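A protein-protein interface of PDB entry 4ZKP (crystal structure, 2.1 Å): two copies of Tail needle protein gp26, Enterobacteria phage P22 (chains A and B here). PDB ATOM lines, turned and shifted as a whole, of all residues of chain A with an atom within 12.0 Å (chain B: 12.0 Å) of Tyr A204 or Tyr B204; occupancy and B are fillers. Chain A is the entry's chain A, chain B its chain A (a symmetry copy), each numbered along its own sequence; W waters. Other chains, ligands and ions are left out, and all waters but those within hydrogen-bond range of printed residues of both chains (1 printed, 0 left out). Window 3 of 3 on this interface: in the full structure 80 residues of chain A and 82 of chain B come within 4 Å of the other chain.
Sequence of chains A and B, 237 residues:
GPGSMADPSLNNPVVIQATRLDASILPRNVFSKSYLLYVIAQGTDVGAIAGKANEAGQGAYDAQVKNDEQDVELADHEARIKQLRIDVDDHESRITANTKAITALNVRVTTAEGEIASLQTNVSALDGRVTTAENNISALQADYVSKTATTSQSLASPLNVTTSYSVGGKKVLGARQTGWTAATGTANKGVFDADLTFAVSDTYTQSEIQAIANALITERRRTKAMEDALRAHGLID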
ATOM      1  N   ALA A 199     -14.037  -8.318  18.251  1.00  0.00           N
ATOM      2  CA  ALA A 199     -13.115  -9.439  18.118  1.00  0.00           C
ATOM      3  C   ALA A 199     -11.737  -9.066  18.653  1.00  0.00           C
ATOM      4  O   ALA A 199     -11.208  -8.001  18.334  1.00  0.00           O
ATOM      5  CB  ALA A 199     -13.020  -9.881  16.666  1.00  0.00           C
ATOM      6  N   VAL A 200     -11.161  -9.945  19.469  1.00  0.00           N
ATOM      7  CA  VAL A 200      -9.825  -9.727  20.014  1.00  0.00           C
ATOM      8  C   VAL A 200      -8.975 -10.980  19.828  1.00  0.00           C
ATOM      9  O   VAL A 200      -9.148 -11.969  20.540  1.00  0.00           O
ATOM     10  CB  VAL A 200      -9.877  -9.326  21.504  1.00  0.00           C
ATOM     11  CG1 VAL A 200      -8.482  -8.987  22.008  1.00  0.00           C
ATOM     12  CG2 VAL A 200     -10.818  -8.150  21.719  1.00  0.00           C
ATOM     13  N   SER A 201      -8.060 -10.931  18.866  1.00  0.00           N
ATOM     14  CA  SER A 201      -7.190 -12.065  18.569  1.00  0.00           C
ATOM     15  C   SER A 201      -6.024 -12.129  19.550  1.00  0.00           C
ATOM     16  O   SER A 201      -5.839 -11.227  20.366  1.00  0.00           O
ATOM     17  CB  SER A 201      -6.670 -11.984  17.133  1.00  0.00           C
ATOM     18  OG  SER A 201      -7.735 -11.797  16.218  1.00  0.00           O
ATOM     19  N   ASP A 202      -5.238 -13.199  19.464  1.00  0.00           N
ATOM     20  CA  ASP A 202      -4.087 -13.365  20.345  1.00  0.00           C
ATOM     21  C   ASP A 202      -2.864 -12.613  19.822  1.00  0.00           C
ATOM     22  O   ASP A 202      -1.865 -12.468  20.527  1.00  0.00           O
ATOM     23  CB  ASP A 202      -3.759 -14.851  20.528  1.00  0.00           C
ATOM     24  CG  ASP A 202      -3.717 -15.610  19.216  1.00  0.00           C
ATOM     25  OD1 ASP A 202      -3.624 -14.967  18.150  1.00  0.00           O
ATOM     26  OD2 ASP A 202      -3.777 -16.857  19.253  1.00  0.00           O
ATOM     27  N   THR A 203      -2.951 -12.136  18.585  1.00  0.00           N
ATOM     28  CA  THR A 203      -1.899 -11.310  18.004  1.00  0.00           C
ATOM     29  C   THR A 203      -2.460  -9.940  17.641  1.00  0.00           C
ATOM     30  O   THR A 203      -3.661  -9.800  17.409  1.00  0.00           O
ATOM     31  CB  THR A 203      -1.284 -11.962  16.753  1.00  0.00           C
ATOM     32  OG1 THR A 203      -2.299 -12.147  15.758  1.00  0.00           O
ATOM     33  CG2 THR A 203      -0.669 -13.309  17.101  1.00  0.00           C
ATOM     34  N   TYR A 204      -1.592  -8.932  17.601  1.00  0.00           N
ATOM     35  CA  TYR A 204      -2.016  -7.567  17.302  1.00  0.00           C
ATOM     36  C   TYR A 204      -2.670  -7.460  15.928  1.00  0.00           C
ATOM     37  O   TYR A 204      -2.073  -7.819  14.913  1.00  0.00           O
ATOM     38  CB  TYR A 204      -0.830  -6.603  17.389  1.00  0.00           C
ATOM     39  CG  TYR A 204      -1.213  -5.154  17.187  1.00  0.00           C
ATOM     40  CD1 TYR A 204      -1.766  -4.410  18.222  1.00  0.00           C
ATOM     41  CD2 TYR A 204      -1.025  -4.530  15.960  1.00  0.00           C
ATOM     42  CE1 TYR A 204      -2.119  -3.084  18.039  1.00  0.00           C
ATOM     43  CE2 TYR A 204      -1.376  -3.207  15.769  1.00  0.00           C
ATOM     44  CZ  TYR A 204      -1.921  -2.489  16.811  1.00  0.00           C
ATOM     45  OH  TYR A 204      -2.270  -1.172  16.624  1.00  0.00           O
ATOM     46  N   THR A 205      -3.902  -6.961  15.911  1.00  0.00           N
ATOM     47  CA  THR A 205      -4.631  -6.727  14.671  1.00  0.00           C
ATOM     48  C   THR A 205      -5.153  -5.294  14.631  1.00  0.00           C
ATOM     49  O   THR A 205      -6.060  -4.938  15.383  1.00  0.00           O
ATOM     50  CB  THR A 205      -5.803  -7.711  14.510  1.00  0.00           C
ATOM     51  OG1 THR A 205      -5.333  -9.050  14.704  1.00  0.00           O
ATOM     52  CG2 THR A 205      -6.411  -7.593  13.120  1.00  0.00           C
ATOM     53  N   GLN A 206      -4.563  -4.477  13.760  1.00  0.00           N
ATOM     54  CA  GLN A 206      -4.918  -3.065  13.630  1.00  0.00           C
ATOM     55  C   GLN A 206      -6.418  -2.820  13.469  1.00  0.00           C
ATOM     56  O   GLN A 206      -6.975  -1.914  14.091  1.00  0.00           O
ATOM     57  CB  GLN A 206      -4.179  -2.446  12.440  1.00  0.00           C
ATOM     58  CG  GLN A 206      -4.585  -1.009  12.145  1.00  0.00           C
ATOM     59  CD  GLN A 206      -3.787  -0.394  11.013  1.00  0.00           C
ATOM     60  OE1 GLN A 206      -3.688  -0.965   9.927  1.00  0.00           O
ATOM     61  NE2 GLN A 206      -3.221   0.781  11.259  1.00  0.00           N
ATOM     62  N   SER A 207      -7.068  -3.630  12.639  1.00  0.00           N
ATOM     63  CA  SER A 207      -8.487  -3.452  12.350  1.00  0.00           C
ATOM     64  C   SER A 207      -9.353  -3.687  13.585  1.00  0.00           C
ATOM     65  O   SER A 207     -10.430  -3.106  13.716  1.00  0.00           O
ATOM     66  CB  SER A 207      -8.920  -4.385  11.217  1.00  0.00           C
ATOM     67  OG  SER A 207      -8.990  -5.729  11.658  1.00  0.00           O
ATOM     68  N   GLU A 208      -8.881  -4.539  14.490  1.00  0.00           N
ATOM     69  CA  GLU A 208      -9.621  -4.837  15.711  1.00  0.00           C
ATOM     70  C   GLU A 208      -9.497  -3.705  16.727  1.00  0.00           C
ATOM     71  O   GLU A 208     -10.421  -3.450  17.499  1.00  0.00           O
ATOM     72  CB  GLU A 208      -9.133  -6.149  16.328  1.00  0.00           C
ATOM     73  CG  GLU A 208      -9.326  -7.363  15.438  1.00  0.00           C
ATOM     74  CD  GLU A 208      -8.825  -8.642  16.080  1.00  0.00           C
ATOM     75  OE1 GLU A 208      -8.023  -8.556  17.035  1.00  0.00           O
ATOM     76  OE2 GLU A 208      -9.230  -9.735  15.628  1.00  0.00           O
ATOM     77  N   ILE A 209      -8.353  -3.028  16.721  1.00  0.00           N
ATOM     78  CA  ILE A 209      -8.123  -1.917  17.633  1.00  0.00           C
ATOM     79  C   ILE A 209      -8.831  -0.678  17.099  1.00  0.00           C
ATOM     80  O   ILE A 209      -9.309   0.160  17.865  1.00  0.00           O
ATOM     81  CB  ILE A 209      -6.618  -1.661  17.829  1.00  0.00           C
ATOM     82  CG1 ILE A 209      -5.908  -2.952  18.244  1.00  0.00           C
ATOM     83  CG2 ILE A 209      -6.386  -0.563  18.859  1.00  0.00           C
ATOM     84  CD1 ILE A 209      -6.064  -3.296  19.712  1.00  0.00           C
ATOM     85  N   GLN A 210      -8.905  -0.579  15.776  1.00  0.00           N
ATOM     86  CA  GLN A 210      -9.625   0.504  15.122  1.00  0.00           C
ATOM     87  C   GLN A 210     -11.115   0.421  15.432  1.00  0.00           C
ATOM     88  O   GLN A 210     -11.766   1.438  15.667  1.00  0.00           O
ATOM     89  CB  GLN A 210      -9.396   0.465  13.609  1.00  0.00           C
ATOM     90  CG  GLN A 210      -8.054   1.029  13.170  1.00  0.00           C
ATOM     91  CD  GLN A 210      -7.776   0.795  11.698  1.00  0.00           C
ATOM     92  OE1 GLN A 210      -8.393  -0.065  11.067  1.00  0.00           O
ATOM     93  NE2 GLN A 210      -6.843   1.559  11.143  1.00  0.00           N
ATOM     94  N   ALA A 211     -11.645  -0.799  15.430  1.00  0.00           N
ATOM     95  CA  ALA A 211     -13.057  -1.035  15.706  1.00  0.00           C
ATOM     96  C   ALA A 211     -13.420  -0.602  17.122  1.00  0.00           C
ATOM     97  O   ALA A 211     -14.477  -0.014  17.350  1.00  0.00           O
ATOM     98  CB  ALA A 211     -13.400  -2.502  15.494  1.00  0.00           C
ATOM     99  N   ILE A 212     -12.539  -0.906  18.070  1.00  0.00           N
ATOM    100  CA  ILE A 212     -12.735  -0.516  19.461  1.00  0.00           C
ATOM    101  C   ILE A 212     -12.697   1.003  19.586  1.00  0.00           C
ATOM    102  O   ILE A 212     -13.546   1.602  20.249  1.00  0.00           O
ATOM    103  CB  ILE A 212     -11.683  -1.172  20.376  1.00  0.00           C
ATOM    104  CG1 ILE A 212     -11.941  -2.675  20.489  1.00  0.00           C
ATOM    105  CG2 ILE A 212     -11.690  -0.523  21.754  1.00  0.00           C
ATOM    106  CD1 ILE A 212     -10.768  -3.459  21.037  1.00  0.00           C
ATOM    107  N   ALA A 213     -11.711   1.621  18.943  1.00  0.00           N
ATOM    108  CA  ALA A 213     -11.548   3.069  18.991  1.00  0.00           C
ATOM    109  C   ALA A 213     -12.729   3.769  18.327  1.00  0.00           C
ATOM    110  O   ALA A 213     -13.182   4.815  18.792  1.00  0.00           O
ATOM    111  CB  ALA A 213     -10.244   3.479  18.326  1.00  0.00           C
ATOM    112  N   ASN A 214     -13.216   3.188  17.236  1.00  0.00           N
ATOM    113  CA  ASN A 214     -14.356   3.738  16.510  1.00  0.00           C
ATOM    114  C   ASN A 214     -15.613   3.730  17.374  1.00  0.00           C
ATOM    115  O   ASN A 214     -16.389   4.686  17.366  1.00  0.00           O
ATOM    116  CB  ASN A 214     -14.603   2.949  15.222  1.00  0.00           C
ATOM    117  CG  ASN A 214     -13.678   3.364  14.096  1.00  0.00           C
ATOM    118  OD1 ASN A 214     -12.849   4.261  14.255  1.00  0.00           O
ATOM    119  ND2 ASN A 214     -13.813   2.711  12.948  1.00  0.00           N
ATOM    120  N   PHE B 198      -8.111   8.776  17.746  1.00  0.00           N
ATOM    121  CA  PHE B 198      -7.031   7.924  18.233  1.00  0.00           C
ATOM    122  C   PHE B 198      -6.194   7.358  17.093  1.00  0.00           C
ATOM    123  O   PHE B 198      -6.729   6.849  16.108  1.00  0.00           O
ATOM    124  CB  PHE B 198      -7.600   6.781  19.078  1.00  0.00           C
ATOM    125  CG  PHE B 198      -8.609   7.228  20.094  1.00  0.00           C
ATOM    126  CD1 PHE B 198      -8.205   7.674  21.340  1.00  0.00           C
ATOM    127  CD2 PHE B 198      -9.965   7.205  19.803  1.00  0.00           C
ATOM    128  CE1 PHE B 198      -9.128   8.090  22.274  1.00  0.00           C
ATOM    129  CE2 PHE B 198     -10.895   7.619  20.736  1.00  0.00           C
ATOM    130  CZ  PHE B 198     -10.476   8.062  21.973  1.00  0.00           C
ATOM    131  N   ALA B 199      -4.876   7.451  17.236  1.00  0.00           N
ATOM    132  CA  ALA B 199      -3.956   6.863  16.271  1.00  0.00           C
ATOM    133  C   ALA B 199      -3.839   5.359  16.489  1.00  0.00           C
ATOM    134  O   ALA B 199      -3.668   4.901  17.618  1.00  0.00           O
ATOM    135  CB  ALA B 199      -2.589   7.523  16.368  1.00  0.00           C
ATOM    136  N   VAL B 200      -3.936   4.594  15.404  1.00  0.00           N
ATOM    137  CA  VAL B 200      -3.798   3.144  15.471  1.00  0.00           C
ATOM    138  C   VAL B 200      -2.827   2.661  14.398  1.00  0.00           C
ATOM    139  O   VAL B 200      -3.168   2.614  13.216  1.00  0.00           O
ATOM    140  CB  VAL B 200      -5.162   2.434  15.324  1.00  0.00           C
ATOM    141  CG1 VAL B 200      -5.001   0.935  15.522  1.00  0.00           C
ATOM    142  CG2 VAL B 200      -6.176   2.993  16.311  1.00  0.00           C
ATOM    143  N   SER B 201      -1.617   2.308  14.817  1.00  0.00           N
ATOM    144  CA  SER B 201      -0.585   1.844  13.895  1.00  0.00           C
ATOM    145  C   SER B 201      -0.790   0.376  13.539  1.00  0.00           C
ATOM    146  O   SER B 201      -1.655  -0.293  14.106  1.00  0.00           O
ATOM    147  CB  SER B 201       0.807   2.053  14.494  1.00  0.00           C
ATOM    148  OG  SER B 201       0.970   3.386  14.946  1.00  0.00           O
ATOM    149  N   ASP B 202       0.008  -0.123  12.599  1.00  0.00           N
ATOM    150  CA  ASP B 202      -0.092  -1.518  12.183  1.00  0.00           C
ATOM    151  C   ASP B 202       0.683  -2.443  13.120  1.00  0.00           C
ATOM    152  O   ASP B 202       0.553  -3.665  13.049  1.00  0.00           O
ATOM    153  CB  ASP B 202       0.401  -1.684  10.742  1.00  0.00           C
ATOM    154  CG  ASP B 202       1.731  -1.002  10.491  1.00  0.00           C
ATOM    155  OD1 ASP B 202       2.433  -0.672  11.469  1.00  0.00           O
ATOM    156  OD2 ASP B 202       2.076  -0.795   9.309  1.00  0.00           O
ATOM    157  N   THR B 203       1.491  -1.851  13.995  1.00  0.00           N
ATOM    158  CA  THR B 203       2.206  -2.610  15.014  1.00  0.00           C
ATOM    159  C   THR B 203       1.784  -2.140  16.401  1.00  0.00           C
ATOM    160  O   THR B 203       1.341  -1.002  16.564  1.00  0.00           O
ATOM    161  CB  THR B 203       3.732  -2.470  14.866  1.00  0.00           C
ATOM    162  OG1 THR B 203       4.104  -1.093  15.000  1.00  0.00           O
ATOM    163  CG2 THR B 203       4.186  -2.985  13.509  1.00  0.00           C
ATOM    164  N   TYR B 204       1.912  -3.016  17.393  1.00  0.00           N
ATOM    165  CA  TYR B 204       1.505  -2.694  18.758  1.00  0.00           C
ATOM    166  C   TYR B 204       2.266  -1.493  19.311  1.00  0.00           C
ATOM    167  O   TYR B 204       3.497  -1.488  19.356  1.00  0.00           O
ATOM    168  CB  TYR B 204       1.700  -3.901  19.678  1.00  0.00           C
ATOM    169  CG  TYR B 204       1.208  -3.672  21.090  1.00  0.00           C
ATOM    170  CD1 TYR B 204      -0.142  -3.777  21.401  1.00  0.00           C
ATOM    171  CD2 TYR B 204       2.092  -3.345  22.110  1.00  0.00           C
ATOM    172  CE1 TYR B 204      -0.595  -3.566  22.692  1.00  0.00           C
ATOM    173  CE2 TYR B 204       1.648  -3.132  23.401  1.00  0.00           C
ATOM    174  CZ  TYR B 204       0.304  -3.243  23.686  1.00  0.00           C
ATOM    175  OH  TYR B 204      -0.140  -3.033  24.971  1.00  0.00           O
ATOM    176  N   THR B 205       1.519  -0.479  19.735  1.00  0.00           N
ATOM    177  CA  THR B 205       2.094   0.707  20.358  1.00  0.00           C
ATOM    178  C   THR B 205       1.407   0.984  21.693  1.00  0.00           C
ATOM    179  O   THR B 205       0.240   1.373  21.725  1.00  0.00           O
ATOM    180  CB  THR B 205       1.972   1.940  19.447  1.00  0.00           C
ATOM    181  OG1 THR B 205       2.477   1.622  18.144  1.00  0.00           O
ATOM    182  CG2 THR B 205       2.765   3.106  20.018  1.00  0.00           C
ATOM    183  N   GLN B 206       2.135   0.765  22.785  1.00  0.00           N
ATOM    184  CA  GLN B 206       1.611   0.942  24.139  1.00  0.00           C
ATOM    185  C   GLN B 206       0.931   2.292  24.363  1.00  0.00           C
ATOM    186  O   GLN B 206      -0.138   2.361  24.970  1.00  0.00           O
ATOM    187  CB  GLN B 206       2.735   0.770  25.163  1.00  0.00           C
ATOM    188  CG  GLN B 206       2.311   1.065  26.595  1.00  0.00           C
ATOM    189  CD  GLN B 206       3.419   0.816  27.599  1.00  0.00           C
ATOM    190  OE1 GLN B 206       4.532   1.317  27.448  1.00  0.00           O
ATOM    191  NE2 GLN B 206       3.114   0.045  28.636  1.00  0.00           N
ATOM    192  N   SER B 207       1.551   3.360  23.869  1.00  0.00           N
ATOM    193  CA  SER B 207       1.036   4.708  24.079  1.00  0.00           C
ATOM    194  C   SER B 207      -0.311   4.917  23.392  1.00  0.00           C
ATOM    195  O   SER B 207      -1.130   5.715  23.847  1.00  0.00           O
ATOM    196  CB  SER B 207       2.046   5.746  23.584  1.00  0.00           C
ATOM    197  OG  SER B 207       2.090   5.785  22.169  1.00  0.00           O
ATOM    198  N   GLU B 208      -0.540   4.198  22.297  1.00  0.00           N
ATOM    199  CA  GLU B 208      -1.793   4.312  21.561  1.00  0.00           C
ATOM    200  C   GLU B 208      -2.924   3.572  22.270  1.00  0.00           C
ATOM    201  O   GLU B 208      -4.082   3.981  22.202  1.00  0.00           O
ATOM    202  CB  GLU B 208      -1.631   3.777  20.137  1.00  0.00           C
ATOM    203  CG  GLU B 208      -0.610   4.530  19.303  1.00  0.00           C
ATOM    204  CD  GLU B 208      -0.472   3.968  17.902  1.00  0.00           C
ATOM    205  OE1 GLU B 208      -0.883   2.808  17.683  1.00  0.00           O
ATOM    206  OE2 GLU B 208       0.051   4.682  17.022  1.00  0.00           O
ATOM    207  N   ILE B 209      -2.581   2.484  22.952  1.00  0.00           N
ATOM    208  CA  ILE B 209      -3.569   1.702  23.683  1.00  0.00           C
ATOM    209  C   ILE B 209      -3.883   2.400  25.000  1.00  0.00           C
ATOM    210  O   ILE B 209      -5.008   2.342  25.498  1.00  0.00           O
ATOM    211  CB  ILE B 209      -3.077   0.262  23.916  1.00  0.00           C
ATOM    212  CG1 ILE B 209      -2.650  -0.374  22.590  1.00  0.00           C
ATOM    213  CG2 ILE B 209      -4.156  -0.574  24.592  1.00  0.00           C
ATOM    214  CD1 ILE B 209      -3.805  -0.880  21.749  1.00  0.00           C
ATOM    215  N   GLN B 210      -2.877   3.071  25.553  1.00  0.00           N
ATOM    216  CA  GLN B 210      -3.049   3.858  26.766  1.00  0.00           C
ATOM    217  C   GLN B 210      -3.999   5.024  26.519  1.00  0.00           C
ATOM    218  O   GLN B 210      -4.837   5.341  27.363  1.00  0.00           O
ATOM    219  CB  GLN B 210      -1.698   4.373  27.267  1.00  0.00           C
ATOM    220  CG  GLN B 210      -0.871   3.331  28.004  1.00  0.00           C
ATOM    221  CD  GLN B 210       0.535   3.811  28.310  1.00  0.00           C
ATOM    222  OE1 GLN B 210       1.024   4.763  27.701  1.00  0.00           O
ATOM    223  NE2 GLN B 210       1.191   3.152  29.258  1.00  0.00           N
ATOM    224  N   ALA B 211      -3.860   5.654  25.357  1.00  0.00           N
ATOM    225  CA  ALA B 211      -4.695   6.789  24.982  1.00  0.00           C
ATOM    226  C   ALA B 211      -6.161   6.382  24.877  1.00  0.00           C
ATOM    227  O   ALA B 211      -7.052   7.116  25.306  1.00  0.00           O
ATOM    228  CB  ALA B 211      -4.215   7.389  23.669  1.00  0.00           C
ATOM    229  N   ILE B 212      -6.402   5.211  24.298  1.00  0.00           N
ATOM    230  CA  ILE B 212      -7.752   4.675  24.167  1.00  0.00           C
ATOM    231  C   ILE B 212      -8.327   4.375  25.547  1.00  0.00           C
ATOM    232  O   ILE B 212      -9.473   4.722  25.842  1.00  0.00           O
ATOM    233  CB  ILE B 212      -7.769   3.420  23.277  1.00  0.00           C
ATOM    234  CG1 ILE B 212      -7.499   3.798  21.820  1.00  0.00           C
ATOM    235  CG2 ILE B 212      -9.100   2.689  23.401  1.00  0.00           C
ATOM    236  CD1 ILE B 212      -7.118   2.625  20.942  1.00  0.00           C
ATOM    237  N   ALA B 213      -7.526   3.732  26.391  1.00  0.00           N
ATOM    238  CA  ALA B 213      -7.955   3.368  27.736  1.00  0.00           C
ATOM    239  C   ALA B 213      -8.219   4.613  28.575  1.00  0.00           C
ATOM    240  O   ALA B 213      -9.155   4.647  29.374  1.00  0.00           O
ATOM    241  CB  ALA B 213      -6.913   2.485  28.405  1.00  0.00           C
ATOM    242  N   ASN B 214      -7.382   5.630  28.394  1.00  0.00           N
ATOM    243  CA  ASN B 214      -7.527   6.889  29.115  1.00  0.00           C
ATOM    244  C   ASN B 214      -8.838   7.582  28.756  1.00  0.00           C
ATOM    245  O   ASN B 214      -9.519   8.130  29.621  1.00  0.00           O
ATOM    246  CB  ASN B 214      -6.347   7.817  28.817  1.00  0.00           C
ATOM    247  CG  ASN B 214      -5.118   7.481  29.637  1.00  0.00           C
ATOM    248  OD1 ASN B 214      -5.134   6.560  30.455  1.00  0.00           O
ATOM    249  ND2 ASN B 214      -4.041   8.228  29.422  1.00  0.00           N
HETATM  250  O   HOH W   1      -5.193   4.404  12.049  1.00  0.00           O
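Among the printed residues, pairs that only touch across the chains: Tyr A204 with Val B200, Tyr A204 with Asp B202, Tyr A204 with Thr B203, Tyr A204 with Tyr B204, Gln A206 with Asp B202, Ile A209 with Val B200, Ile A209 with Ile B209, Ile A209 with Ile B212 and Gln A210 with Val B200.
Water W1 bridges O of Val B200 and NE2 of Gln A210.
Of the 17 printed residues of chain B, 7 touch a printed residue of chain A. Hydrophobic or aromatic side chains of chain B that line the printed part of chain A: Val B200, Tyr B204, Ile B209 and Ile B212. Of the 16 printed residues of chain A, 4 touch a printed residue of chain B. Along chain A the printed residues that touch a printed residue of chain B span positions 204 to 210. Among the printed residues, 12 pairs touch across the chains.
The backbone carbonyl oxygen (O) of Gln A210 lies close to the side-chain amide oxygen (OD1) of Asn A214 (3.3 Å). The side-chain hydroxyl (OG) of Ser B201 is in hydrogen-bond range of the side-chain carboxylate (OE2) of Glu B208 (2.6 Å). O of Thr B203 sits at hydrogen-bond distance from OG1 of Thr B205 (3.3 Å).
Tyr A204 touches Asp B202, but with the chains exchanged Asp A202 does not touch Tyr B204 (8.9 Å). Tyr B204 touches its own counterpart, Tyr A204. Gln A206 touches Val B200, but with the chains exchanged Val A200 does not touch Gln B206 (14.3 Å). Gln A210 touches Val B200, but with the chains exchanged Val A200 does not touch Gln B210 (13.8 Å). 16 positions are printed for both chains. Of the 12 pairs that touch across the chains among the printed residues, 2 have their exchanged pair printed and touching as well.
The side-chain hydroxyl (OH) of Tyr A204 sits at hydrogen-bond distance from the backbone carbonyl oxygen (O) of Ser B201. The side-chain amide nitrogen (NE2) of Gln A206 is in hydrogen-bond range of the backbone carbonyl oxygen (O) of Val B200, at 2.7 Å. The backbone carbonyl oxygen (O) of Ser B201 lies close to the side-chain amide nitrogen (NE2) of Gln A206 (3.4 Å).
Of chain A, only Tyr A204 comes within 4 Å of Tyr B204. No residue of chain B comes within 4 Å of Ser A201. No residue of chain B comes within 4 Å of Thr A203. Thr A205 touches none of the printed residues of chain B. Val B200 touches four residues of chain A. Of chain A, only Tyr A204 and Gln A206 come within 4 Å of Asp B202. No residue of chain A comes within 4 Å of Gln B206. Of chain A, only Ile A209 (3.9 Å) comes within 4 Å of Ile B209. Of the printed residues of chain A, Ile B212 touches Ile A209 (3.9 Å). Of the printed residues of chain B, Gln A210 touches Val B200. The nearest residue of chain B that does not touch Tyr A204 is Glu B208 (4.3 Å). The nearest residue of chain A that does not touch Tyr B204 is Ile A209 (6.2 Å).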
